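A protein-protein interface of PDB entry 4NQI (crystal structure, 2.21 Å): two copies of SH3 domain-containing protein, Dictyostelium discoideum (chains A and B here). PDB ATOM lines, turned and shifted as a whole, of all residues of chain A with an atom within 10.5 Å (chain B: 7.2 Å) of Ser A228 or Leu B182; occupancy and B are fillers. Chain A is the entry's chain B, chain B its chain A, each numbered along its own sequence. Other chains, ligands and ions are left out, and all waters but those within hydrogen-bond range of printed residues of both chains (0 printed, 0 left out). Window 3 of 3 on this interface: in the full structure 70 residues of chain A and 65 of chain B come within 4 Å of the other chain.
O of Ser A226 lies within hydrogen-bond range of NH1 of Arg B185, 3.2 Å away. The side-chain carboxylate of Asp A73 is in salt-bridge range of the guanidinium group of Arg B185, at 2.6 Å.
O of Asp A222 is in hydrogen-bond range of OG of Ser A226. The backbone carbonyl oxygen (O) of Ile A224 sits at hydrogen-bond distance from the side-chain amide nitrogen (NE2) of Gln A227 (3.0 Å). NE2 of Gln A229 sits at hydrogen-bond distance from OG of Ser A226 (3.4 Å).
Among the printed residues, pairs that only touch across the chains: Phe A74 with Arg B185 (3.3 Å), Phe A74 with His B188 (3.4 Å), Gln A227 with Leu B182 (3.7 Å), Gln A227 with Arg B185 (3.4 Å), Gln A227 with Arg B186 (3.5 Å), Ser A228 with Leu B182 (3.7 Å), Gln A229 with Arg B185 (3.7 Å), Leu A230 with Arg B178 (3.5 Å), Leu A230 with Val B181 (3.5 Å), Pro A231 with Arg B185 (3.9 Å) and Met A234 with Val B181 (3.9 Å).
Of the printed residues of chain B, Asp A73 touches Arg B185. Of the printed residues of chain B, Ser A226 touches Arg B185 (3.2 Å). Of the printed residues of chain B, Gln A227 touches Leu B182, Arg B185 and Arg B186. Ser A228 touches just one residue of chain B: Leu B182. Of the printed residues of chain B, Leu A230 touches Arg B178 (3.5 Å) and Val B181 (3.5 Å). Val B180 touches none of the printed residues of chain A. Of chain A, only Leu A230 and Met A234 come within 4 Å of Val B181. Leu B182 touches two residues of chain A. Printed residues of chain A within 4 Å of Arg B185: Asp A73, Phe A74, Ser A226, Gln A227, Gln A229 and Pro A231. Of chain A, only Gln A227 comes within 4 Å of Arg B186. The nearest residue of chain B that does not touch Ser A228 is Arg B185 (5.4 Å). The nearest printed residue of chain A that does not touch Arg B185 is Leu A223 (4.7 Å).
Hydrophobic or aromatic side chains of chain A within 4 Å of the printed part of chain B: Phe A74, Leu A230, Pro A231 and Met A234. Of the 15 printed residues of chain B, 6 touch a printed residue of chain A. Printed residues of chain B that touch a printed residue of chain A: Arg B178, Val B181, Leu B182, Arg B185, Arg B186 and His B188. Among the printed residues, 13 pairs touch across the chains.
No position is printed for both chains. Of the 13 pairs that touch across the chains among the printed residues, none has its exchanged pair printed and touching as well.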
ATOM      1  N   ASP A  73      29.271  -3.279 -27.277  1.00  0.00           N
ATOM      2  CA  ASP A  73      28.447  -2.129 -27.638  1.00  0.00           C
ATOM      3  C   ASP A  73      27.692  -1.536 -26.447  1.00  0.00           C
ATOM      4  O   ASP A  73      27.546  -0.313 -26.349  1.00  0.00           O
ATOM      5  CB  ASP A  73      27.481  -2.476 -28.776  1.00  0.00           C
ATOM      6  CG  ASP A  73      26.873  -3.855 -28.624  1.00  0.00           C
ATOM      7  OD1 ASP A  73      26.925  -4.412 -27.506  1.00  0.00           O
ATOM      8  OD2 ASP A  73      26.338  -4.381 -29.623  1.00  0.00           O
ATOM      9  N   PHE A  74      27.213  -2.395 -25.547  1.00  0.00           N
ATOM     10  CA  PHE A  74      26.560  -1.919 -24.332  1.00  0.00           C
ATOM     11  C   PHE A  74      27.548  -1.104 -23.498  1.00  0.00           C
ATOM     12  O   PHE A  74      27.215  -0.017 -23.013  1.00  0.00           O
ATOM     13  CB  PHE A  74      25.978  -3.081 -23.518  1.00  0.00           C
ATOM     14  CG  PHE A  74      24.589  -3.485 -23.943  1.00  0.00           C
ATOM     15  CD1 PHE A  74      23.493  -2.690 -23.626  1.00  0.00           C
ATOM     16  CD2 PHE A  74      24.375  -4.659 -24.648  1.00  0.00           C
ATOM     17  CE1 PHE A  74      22.212  -3.060 -24.010  1.00  0.00           C
ATOM     18  CE2 PHE A  74      23.097  -5.031 -25.034  1.00  0.00           C
ATOM     19  CZ  PHE A  74      22.017  -4.231 -24.715  1.00  0.00           C
ATOM     20  N   ARG A 221      18.144   2.783 -28.086  1.00  0.00           N
ATOM     21  CA  ARG A 221      17.075   2.131 -28.837  1.00  0.00           C
ATOM     22  C   ARG A 221      17.622   1.039 -29.752  1.00  0.00           C
ATOM     23  O   ARG A 221      17.062  -0.054 -29.827  1.00  0.00           O
ATOM     24  CB  ARG A 221      16.299   3.150 -29.669  1.00  0.00           C
ATOM     25  CG  ARG A 221      14.975   2.623 -30.198  1.00  0.00           C
ATOM     26  CD  ARG A 221      14.447   3.456 -31.356  1.00  0.00           C
ATOM     27  NE  ARG A 221      14.758   4.877 -31.223  1.00  0.00           N
ATOM     28  CZ  ARG A 221      14.103   5.712 -30.423  1.00  0.00           C
ATOM     29  NH1 ARG A 221      13.109   5.266 -29.667  1.00  0.00           N
ATOM     30  NH2 ARG A 221      14.449   6.992 -30.370  1.00  0.00           N
ATOM     31  N   ASP A 222      18.717   1.344 -30.441  1.00  0.00           N
ATOM     32  CA  ASP A 222      19.373   0.367 -31.301  1.00  0.00           C
ATOM     33  C   ASP A 222      19.947  -0.774 -30.463  1.00  0.00           C
ATOM     34  O   ASP A 222      19.913  -1.936 -30.871  1.00  0.00           O
ATOM     35  CB  ASP A 222      20.478   1.037 -32.121  1.00  0.00           C
ATOM     36  CG  ASP A 222      21.058   0.120 -33.180  1.00  0.00           C
ATOM     37  OD1 ASP A 222      20.319  -0.239 -34.122  1.00  0.00           O
ATOM     38  OD2 ASP A 222      22.252  -0.235 -33.078  1.00  0.00           O
ATOM     39  N   LEU A 223      20.467  -0.431 -29.286  1.00  0.00           N
ATOM     40  CA  LEU A 223      20.999  -1.420 -28.350  1.00  0.00           C
ATOM     41  C   LEU A 223      19.895  -2.325 -27.802  1.00  0.00           C
ATOM     42  O   LEU A 223      20.053  -3.547 -27.750  1.00  0.00           O
ATOM     43  CB  LEU A 223      21.719  -0.727 -27.189  1.00  0.00           C
ATOM     44  CG  LEU A 223      23.197  -0.379 -27.364  1.00  0.00           C
ATOM     45  CD1 LEU A 223      23.734   0.322 -26.125  1.00  0.00           C
ATOM     46  CD2 LEU A 223      24.004  -1.630 -27.647  1.00  0.00           C
ATOM     47  N   ILE A 224      18.788  -1.713 -27.388  1.00  0.00           N
ATOM     48  CA  ILE A 224      17.642  -2.440 -26.843  1.00  0.00           C
ATOM     49  C   ILE A 224      17.024  -3.387 -27.880  1.00  0.00           C
ATOM     50  O   ILE A 224      16.716  -4.541 -27.571  1.00  0.00           O
ATOM     51  CB  ILE A 224      16.576  -1.457 -26.304  1.00  0.00           C
ATOM     52  CG1 ILE A 224      17.086  -0.760 -25.037  1.00  0.00           C
ATOM     53  CG2 ILE A 224      15.266  -2.174 -26.015  1.00  0.00           C
ATOM     54  CD1 ILE A 224      16.302   0.493 -24.657  1.00  0.00           C
ATOM     55  N   ASN A 225      16.862  -2.900 -29.108  1.00  0.00           N
ATOM     56  CA  ASN A 225      16.295  -3.707 -30.189  1.00  0.00           C
ATOM     57  C   ASN A 225      17.196  -4.868 -30.634  1.00  0.00           C
ATOM     58  O   ASN A 225      16.759  -5.740 -31.386  1.00  0.00           O
ATOM     59  CB  ASN A 225      15.941  -2.828 -31.398  1.00  0.00           C
ATOM     60  CG  ASN A 225      14.758  -1.908 -31.137  1.00  0.00           C
ATOM     61  OD1 ASN A 225      13.641  -2.367 -30.888  1.00  0.00           O
ATOM     62  ND2 ASN A 225      14.994  -0.603 -31.216  1.00  0.00           N
ATOM     63  N   SER A 226      18.445  -4.875 -30.169  1.00  0.00           N
ATOM     64  CA  SER A 226      19.414  -5.898 -30.562  1.00  0.00           C
ATOM     65  C   SER A 226      19.797  -6.835 -29.415  1.00  0.00           C
ATOM     66  O   SER A 226      20.827  -7.509 -29.482  1.00  0.00           O
ATOM     67  CB  SER A 226      20.684  -5.246 -31.123  1.00  0.00           C
ATOM     68  OG  SER A 226      20.456  -4.670 -32.398  1.00  0.00           O
ATOM     69  N   GLN A 227      18.972  -6.885 -28.373  1.00  0.00           N
ATOM     70  CA  GLN A 227      19.292  -7.685 -27.191  1.00  0.00           C
ATOM     71  C   GLN A 227      19.265  -9.198 -27.440  1.00  0.00           C
ATOM     72  O   GLN A 227      19.904  -9.956 -26.712  1.00  0.00           O
ATOM     73  CB  GLN A 227      18.373  -7.318 -26.016  1.00  0.00           C
ATOM     74  CG  GLN A 227      16.893  -7.595 -26.254  1.00  0.00           C
ATOM     75  CD  GLN A 227      16.022  -7.132 -25.101  1.00  0.00           C
ATOM     76  OE1 GLN A 227      15.867  -7.837 -24.102  1.00  0.00           O
ATOM     77  NE2 GLN A 227      15.444  -5.941 -25.236  1.00  0.00           N
ATOM     78  N   SER A 228      18.542  -9.633 -28.470  1.00  0.00           N
ATOM     79  CA  SER A 228      18.396 -11.064 -28.747  1.00  0.00           C
ATOM     80  C   SER A 228      19.443 -11.636 -29.704  1.00  0.00           C
ATOM     81  O   SER A 228      19.513 -12.853 -29.890  1.00  0.00           O
ATOM     82  CB  SER A 228      16.991 -11.377 -29.269  1.00  0.00           C
ATOM     83  OG  SER A 228      16.045 -11.378 -28.215  1.00  0.00           O
ATOM     84  N   GLN A 229      20.253 -10.773 -30.309  1.00  0.00           N
ATOM     85  CA  GLN A 229      21.280 -11.261 -31.224  1.00  0.00           C
ATOM     86  C   GLN A 229      22.679 -11.233 -30.610  1.00  0.00           C
ATOM     87  O   GLN A 229      23.089 -10.241 -30.000  1.00  0.00           O
ATOM     88  CB  GLN A 229      21.260 -10.492 -32.549  1.00  0.00           C
ATOM     89  CG  GLN A 229      21.594  -9.015 -32.437  1.00  0.00           C
ATOM     90  CD  GLN A 229      22.037  -8.428 -33.765  1.00  0.00           C
ATOM     91  OE1 GLN A 229      22.086  -9.126 -34.780  1.00  0.00           O
ATOM     92  NE2 GLN A 229      22.366  -7.141 -33.763  1.00  0.00           N
ATOM     93  N   LEU A 230      23.401 -12.339 -30.768  1.00  0.00           N
ATOM     94  CA  LEU A 230      24.791 -12.413 -30.343  1.00  0.00           C
ATOM     95  C   LEU A 230      25.656 -11.502 -31.205  1.00  0.00           C
ATOM     96  O   LEU A 230      25.395 -11.337 -32.398  1.00  0.00           O
ATOM     97  CB  LEU A 230      25.312 -13.849 -30.453  1.00  0.00           C
ATOM     98  CG  LEU A 230      25.152 -14.784 -29.257  1.00  0.00           C
ATOM     99  CD1 LEU A 230      25.932 -16.072 -29.482  1.00  0.00           C
ATOM    100  CD2 LEU A 230      25.632 -14.092 -28.006  1.00  0.00           C
ATOM    101  N   PRO A 231      26.691 -10.900 -30.600  1.00  0.00           N
ATOM    102  CA  PRO A 231      27.686 -10.162 -31.383  1.00  0.00           C
ATOM    103  C   PRO A 231      28.355 -11.146 -32.326  1.00  0.00           C
ATOM    104  O   PRO A 231      28.530 -12.301 -31.949  1.00  0.00           O
ATOM    105  CB  PRO A 231      28.688  -9.681 -30.325  1.00  0.00           C
ATOM    106  CG  PRO A 231      27.953  -9.750 -29.028  1.00  0.00           C
ATOM    107  CD  PRO A 231      27.001 -10.892 -29.162  1.00  0.00           C
ATOM    108  N   LEU A 232      28.705 -10.708 -33.529  1.00  0.00           N
ATOM    109  CA  LEU A 232      29.237 -11.600 -34.556  1.00  0.00           C
ATOM    110  C   LEU A 232      30.682 -12.050 -34.244  1.00  0.00           C
ATOM    111  O   LEU A 232      31.160 -13.036 -34.802  1.00  0.00           O
ATOM    112  CB  LEU A 232      29.094 -10.912 -35.918  1.00  0.00           C
ATOM    113  N   MET A 234      31.270 -12.989 -31.226  1.00  0.00           N
ATOM    114  CA  MET A 234      30.834 -14.161 -30.476  1.00  0.00           C
ATOM    115  C   MET A 234      30.663 -15.341 -31.433  1.00  0.00           C
ATOM    116  O   MET A 234      31.351 -16.349 -31.296  1.00  0.00           O
ATOM    117  CB  MET A 234      29.524 -13.897 -29.727  1.00  0.00           C
ATOM    118  CG  MET A 234      29.670 -13.205 -28.385  1.00  0.00           C
ATOM    119  SD  MET A 234      30.248 -14.426 -26.984  1.00  0.00           S
ATOM    120  CE  MET A 234      32.168 -14.166 -27.130  1.00  0.00           C
ATOM    121  N   GLU A 235      29.749 -15.204 -32.395  1.00  0.00           N
ATOM    122  CA  GLU A 235      29.525 -16.220 -33.429  1.00  0.00           C
ATOM    123  C   GLU A 235      30.820 -16.714 -34.081  1.00  0.00           C
ATOM    124  O   GLU A 235      31.090 -17.919 -34.112  1.00  0.00           O
ATOM    125  CB  GLU A 235      28.590 -15.672 -34.514  1.00  0.00           C
ATOM    126  N   THR B  23      31.295 -14.994 -18.029  1.00  0.00           N
ATOM    127  CA  THR B  23      29.999 -14.315 -18.056  1.00  0.00           C
ATOM    128  C   THR B  23      29.139 -14.691 -16.840  1.00  0.00           C
ATOM    129  O   THR B  23      28.410 -13.848 -16.306  1.00  0.00           O
ATOM    130  CB  THR B  23      29.232 -14.608 -19.370  1.00  0.00           C
ATOM    131  OG1 THR B  23      30.018 -14.185 -20.490  1.00  0.00           O
ATOM    132  CG2 THR B  23      27.902 -13.870 -19.400  1.00  0.00           C
ATOM    133  N   LEU B  27      28.058 -11.745 -14.056  1.00  0.00           N
ATOM    134  CA  LEU B  27      26.660 -11.553 -13.679  1.00  0.00           C
ATOM    135  C   LEU B  27      26.439 -11.878 -12.209  1.00  0.00           C
ATOM    136  O   LEU B  27      25.602 -11.262 -11.547  1.00  0.00           O
ATOM    137  CB  LEU B  27      25.745 -12.426 -14.542  1.00  0.00           C
ATOM    138  CG  LEU B  27      25.494 -11.960 -15.976  1.00  0.00           C
ATOM    139  CD1 LEU B  27      24.653 -12.970 -16.749  1.00  0.00           C
ATOM    140  CD2 LEU B  27      24.819 -10.598 -15.972  1.00  0.00           C
ATOM    141  N   LYS B 176      24.743 -23.051 -23.955  1.00  0.00           N
ATOM    142  CA  LYS B 176      24.902 -22.421 -22.646  1.00  0.00           C
ATOM    143  C   LYS B 176      25.638 -21.080 -22.740  1.00  0.00           C
ATOM    144  O   LYS B 176      25.400 -20.177 -21.934  1.00  0.00           O
ATOM    145  CB  LYS B 176      25.624 -23.359 -21.671  1.00  0.00           C
ATOM    146  CG  LYS B 176      24.792 -24.551 -21.192  1.00  0.00           C
ATOM    147  CD  LYS B 176      23.500 -24.100 -20.519  1.00  0.00           C
ATOM    148  CE  LYS B 176      22.615 -25.284 -20.140  1.00  0.00           C
ATOM    149  NZ  LYS B 176      23.112 -26.037 -18.953  1.00  0.00           N
ATOM    150  N   LEU B 177      26.525 -20.952 -23.725  1.00  0.00           N
ATOM    151  CA  LEU B 177      27.204 -19.683 -23.970  1.00  0.00           C
ATOM    152  C   LEU B 177      26.220 -18.641 -24.492  1.00  0.00           C
ATOM    153  O   LEU B 177      26.162 -17.523 -23.972  1.00  0.00           O
ATOM    154  CB  LEU B 177      28.363 -19.850 -24.958  1.00  0.00           C
ATOM    155  CG  LEU B 177      28.988 -18.525 -25.418  1.00  0.00           C
ATOM    156  CD1 LEU B 177      29.584 -17.765 -24.240  1.00  0.00           C
ATOM    157  CD2 LEU B 177      30.035 -18.727 -26.507  1.00  0.00           C
ATOM    158  N   ARG B 178      25.456 -19.009 -25.521  1.00  0.00           N
ATOM    159  CA  ARG B 178      24.417 -18.138 -26.066  1.00  0.00           C
ATOM    160  C   ARG B 178      23.451 -17.711 -24.976  1.00  0.00           C
ATOM    161  O   ARG B 178      23.117 -16.533 -24.858  1.00  0.00           O
ATOM    162  CB  ARG B 178      23.620 -18.853 -27.159  1.00  0.00           C
ATOM    163  CG  ARG B 178      24.358 -19.063 -28.461  1.00  0.00           C
ATOM    164  CD  ARG B 178      23.398 -19.482 -29.563  1.00  0.00           C
ATOM    165  NE  ARG B 178      24.113 -19.942 -30.747  1.00  0.00           N
ATOM    166  CZ  ARG B 178      24.640 -21.156 -30.864  1.00  0.00           C
ATOM    167  NH1 ARG B 178      24.530 -22.025 -29.868  1.00  0.00           N
ATOM    168  NH2 ARG B 178      25.279 -21.502 -31.973  1.00  0.00           N
ATOM    169  N   ASP B 179      23.006 -18.685 -24.189  1.00  0.00           N
ATOM    170  CA  ASP B 179      22.040 -18.447 -23.124  1.00  0.00           C
ATOM    171  C   ASP B 179      22.513 -17.375 -22.147  1.00  0.00           C
ATOM    172  O   ASP B 179      21.762 -16.460 -21.805  1.00  0.00           O
ATOM    173  CB  ASP B 179      21.755 -19.744 -22.367  1.00  0.00           C
ATOM    174  CG  ASP B 179      21.056 -20.781 -23.226  1.00  0.00           C
ATOM    175  OD1 ASP B 179      20.332 -20.386 -24.166  1.00  0.00           O
ATOM    176  OD2 ASP B 179      21.224 -21.991 -22.955  1.00  0.00           O
ATOM    177  N   VAL B 180      23.767 -17.486 -21.713  1.00  0.00           N
ATOM    178  CA  VAL B 180      24.291 -16.597 -20.679  1.00  0.00           C
ATOM    179  C   VAL B 180      24.684 -15.212 -21.206  1.00  0.00           C
ATOM    180  O   VAL B 180      24.535 -14.217 -20.493  1.00  0.00           O
ATOM    181  CB  VAL B 180      25.448 -17.255 -19.881  1.00  0.00           C
ATOM    182  CG1 VAL B 180      26.765 -17.157 -20.639  1.00  0.00           C
ATOM    183  CG2 VAL B 180      25.572 -16.627 -18.504  1.00  0.00           C
ATOM    184  N   VAL B 181      25.159 -15.135 -22.449  1.00  0.00           N
ATOM    185  CA  VAL B 181      25.468 -13.837 -23.044  1.00  0.00           C
ATOM    186  C   VAL B 181      24.172 -13.076 -23.322  1.00  0.00           C
ATOM    187  O   VAL B 181      24.114 -11.853 -23.172  1.00  0.00           O
ATOM    188  CB  VAL B 181      26.304 -13.957 -24.340  1.00  0.00           C
ATOM    189  CG1 VAL B 181      26.564 -12.582 -24.933  1.00  0.00           C
ATOM    190  CG2 VAL B 181      27.627 -14.652 -24.062  1.00  0.00           C
ATOM    191  N   LEU B 182      23.131 -13.808 -23.714  1.00  0.00           N
ATOM    192  CA  LEU B 182      21.819 -13.203 -23.927  1.00  0.00           C
ATOM    193  C   LEU B 182      21.200 -12.758 -22.602  1.00  0.00           C
ATOM    194  O   LEU B 182      20.480 -11.757 -22.557  1.00  0.00           O
ATOM    195  CB  LEU B 182      20.875 -14.152 -24.675  1.00  0.00           C
ATOM    196  CG  LEU B 182      21.180 -14.435 -26.151  1.00  0.00           C
ATOM    197  CD1 LEU B 182      19.979 -15.045 -26.863  1.00  0.00           C
ATOM    198  CD2 LEU B 182      21.643 -13.183 -26.872  1.00  0.00           C
ATOM    199  N   MET B 183      21.482 -13.499 -21.529  1.00  0.00           N
ATOM    200  CA  MET B 183      21.048 -13.097 -20.191  1.00  0.00           C
ATOM    201  C   MET B 183      21.647 -11.744 -19.833  1.00  0.00           C
ATOM    202  O   MET B 183      20.971 -10.883 -19.269  1.00  0.00           O
ATOM    203  CB  MET B 183      21.473 -14.125 -19.140  1.00  0.00           C
ATOM    204  CG  MET B 183      20.600 -15.363 -19.060  1.00  0.00           C
ATOM    205  SD  MET B 183      21.215 -16.587 -17.668  1.00  0.00           S
ATOM    206  CE  MET B 183      20.856 -15.471 -16.110  1.00  0.00           C
ATOM    207  N   GLU B 184      22.922 -11.565 -20.170  1.00  0.00           N
ATOM    208  CA  GLU B 184      23.628 -10.321 -19.886  1.00  0.00           C
ATOM    209  C   GLU B 184      23.113  -9.185 -20.768  1.00  0.00           C
ATOM    210  O   GLU B 184      22.978  -8.044 -20.310  1.00  0.00           O
ATOM    211  CB  GLU B 184      25.135 -10.507 -20.078  1.00  0.00           C
ATOM    212  CG  GLU B 184      25.980  -9.356 -19.555  1.00  0.00           C
ATOM    213  CD  GLU B 184      27.457  -9.703 -19.474  1.00  0.00           C
ATOM    214  OE1 GLU B 184      28.037 -10.105 -20.506  1.00  0.00           O
ATOM    215  OE2 GLU B 184      28.036  -9.580 -18.375  1.00  0.00           O
ATOM    216  N   ARG B 185      22.818  -9.500 -22.026  1.00  0.00           N
ATOM    217  CA  ARG B 185      22.296  -8.501 -22.953  1.00  0.00           C
ATOM    218  C   ARG B 185      20.913  -8.017 -22.528  1.00  0.00           C
ATOM    219  O   ARG B 185      20.646  -6.813 -22.526  1.00  0.00           O
ATOM    220  CB  ARG B 185      22.257  -9.049 -24.381  1.00  0.00           C
ATOM    221  CG  ARG B 185      23.636  -9.252 -24.989  1.00  0.00           C
ATOM    222  CD  ARG B 185      23.595  -9.188 -26.506  1.00  0.00           C
ATOM    223  NE  ARG B 185      24.744  -8.460 -27.039  1.00  0.00           N
ATOM    224  CZ  ARG B 185      24.668  -7.283 -27.651  1.00  0.00           C
ATOM    225  NH1 ARG B 185      23.493  -6.696 -27.832  1.00  0.00           N
ATOM    226  NH2 ARG B 185      25.771  -6.696 -28.094  1.00  0.00           N
ATOM    227  N   ARG B 186      20.039  -8.954 -22.166  1.00  0.00           N
ATOM    228  CA  ARG B 186      18.705  -8.601 -21.687  1.00  0.00           C
ATOM    229  C   ARG B 186      18.773  -7.727 -20.436  1.00  0.00           C
ATOM    230  O   ARG B 186      17.973  -6.805 -20.275  1.00  0.00           O
ATOM    231  CB  ARG B 186      17.861  -9.852 -21.418  1.00  0.00           C
ATOM    232  CG  ARG B 186      17.424 -10.583 -22.682  1.00  0.00           C
ATOM    233  CD  ARG B 186      16.171 -11.430 -22.454  1.00  0.00           C
ATOM    234  NE  ARG B 186      16.364 -12.455 -21.432  1.00  0.00           N
ATOM    235  CZ  ARG B 186      17.015 -13.599 -21.632  1.00  0.00           C
ATOM    236  NH1 ARG B 186      17.555 -13.864 -22.815  1.00  0.00           N
ATOM    237  NH2 ARG B 186      17.134 -14.474 -20.644  1.00  0.00           N
ATOM    238  N   LYS B 187      19.733  -8.020 -19.559  1.00  0.00           N
ATOM    239  CA  LYS B 187      19.929  -7.246 -18.335  1.00  0.00           C
ATOM    240  C   LYS B 187      20.293  -5.796 -18.640  1.00  0.00           C
ATOM    241  O   LYS B 187      19.726  -4.865 -18.062  1.00  0.00           O
ATOM    242  CB  LYS B 187      21.024  -7.876 -17.472  1.00  0.00           C
ATOM    243  CG  LYS B 187      21.374  -7.068 -16.228  1.00  0.00           C
ATOM    244  CD  LYS B 187      22.397  -7.790 -15.358  1.00  0.00           C
ATOM    245  CE  LYS B 187      22.695  -7.001 -14.092  1.00  0.00           C
ATOM    246  NZ  LYS B 187      21.473  -6.799 -13.267  1.00  0.00           N
ATOM    247  N   HIS B 188      21.239  -5.610 -19.555  1.00  0.00           N
ATOM    248  CA  HIS B 188      21.696  -4.279 -19.930  1.00  0.00           C
ATOM    249  C   HIS B 188      20.621  -3.516 -20.710  1.00  0.00           C
ATOM    250  O   HIS B 188      20.487  -2.299 -20.568  1.00  0.00           O
ATOM    251  CB  HIS B 188      22.982  -4.380 -20.749  1.00  0.00           C
ATOM    252  CG  HIS B 188      24.154  -4.917 -19.986  1.00  0.00           C
ATOM    253  ND1 HIS B 188      24.186  -4.968 -18.602  1.00  0.00           N
ATOM    254  CD2 HIS B 188      25.332  -5.420 -20.405  1.00  0.00           C
ATOM    255  CE1 HIS B 188      25.334  -5.479 -18.215  1.00  0.00           C
ATOM    256  NE2 HIS B 188      26.057  -5.765 -19.287  1.00  0.00           N
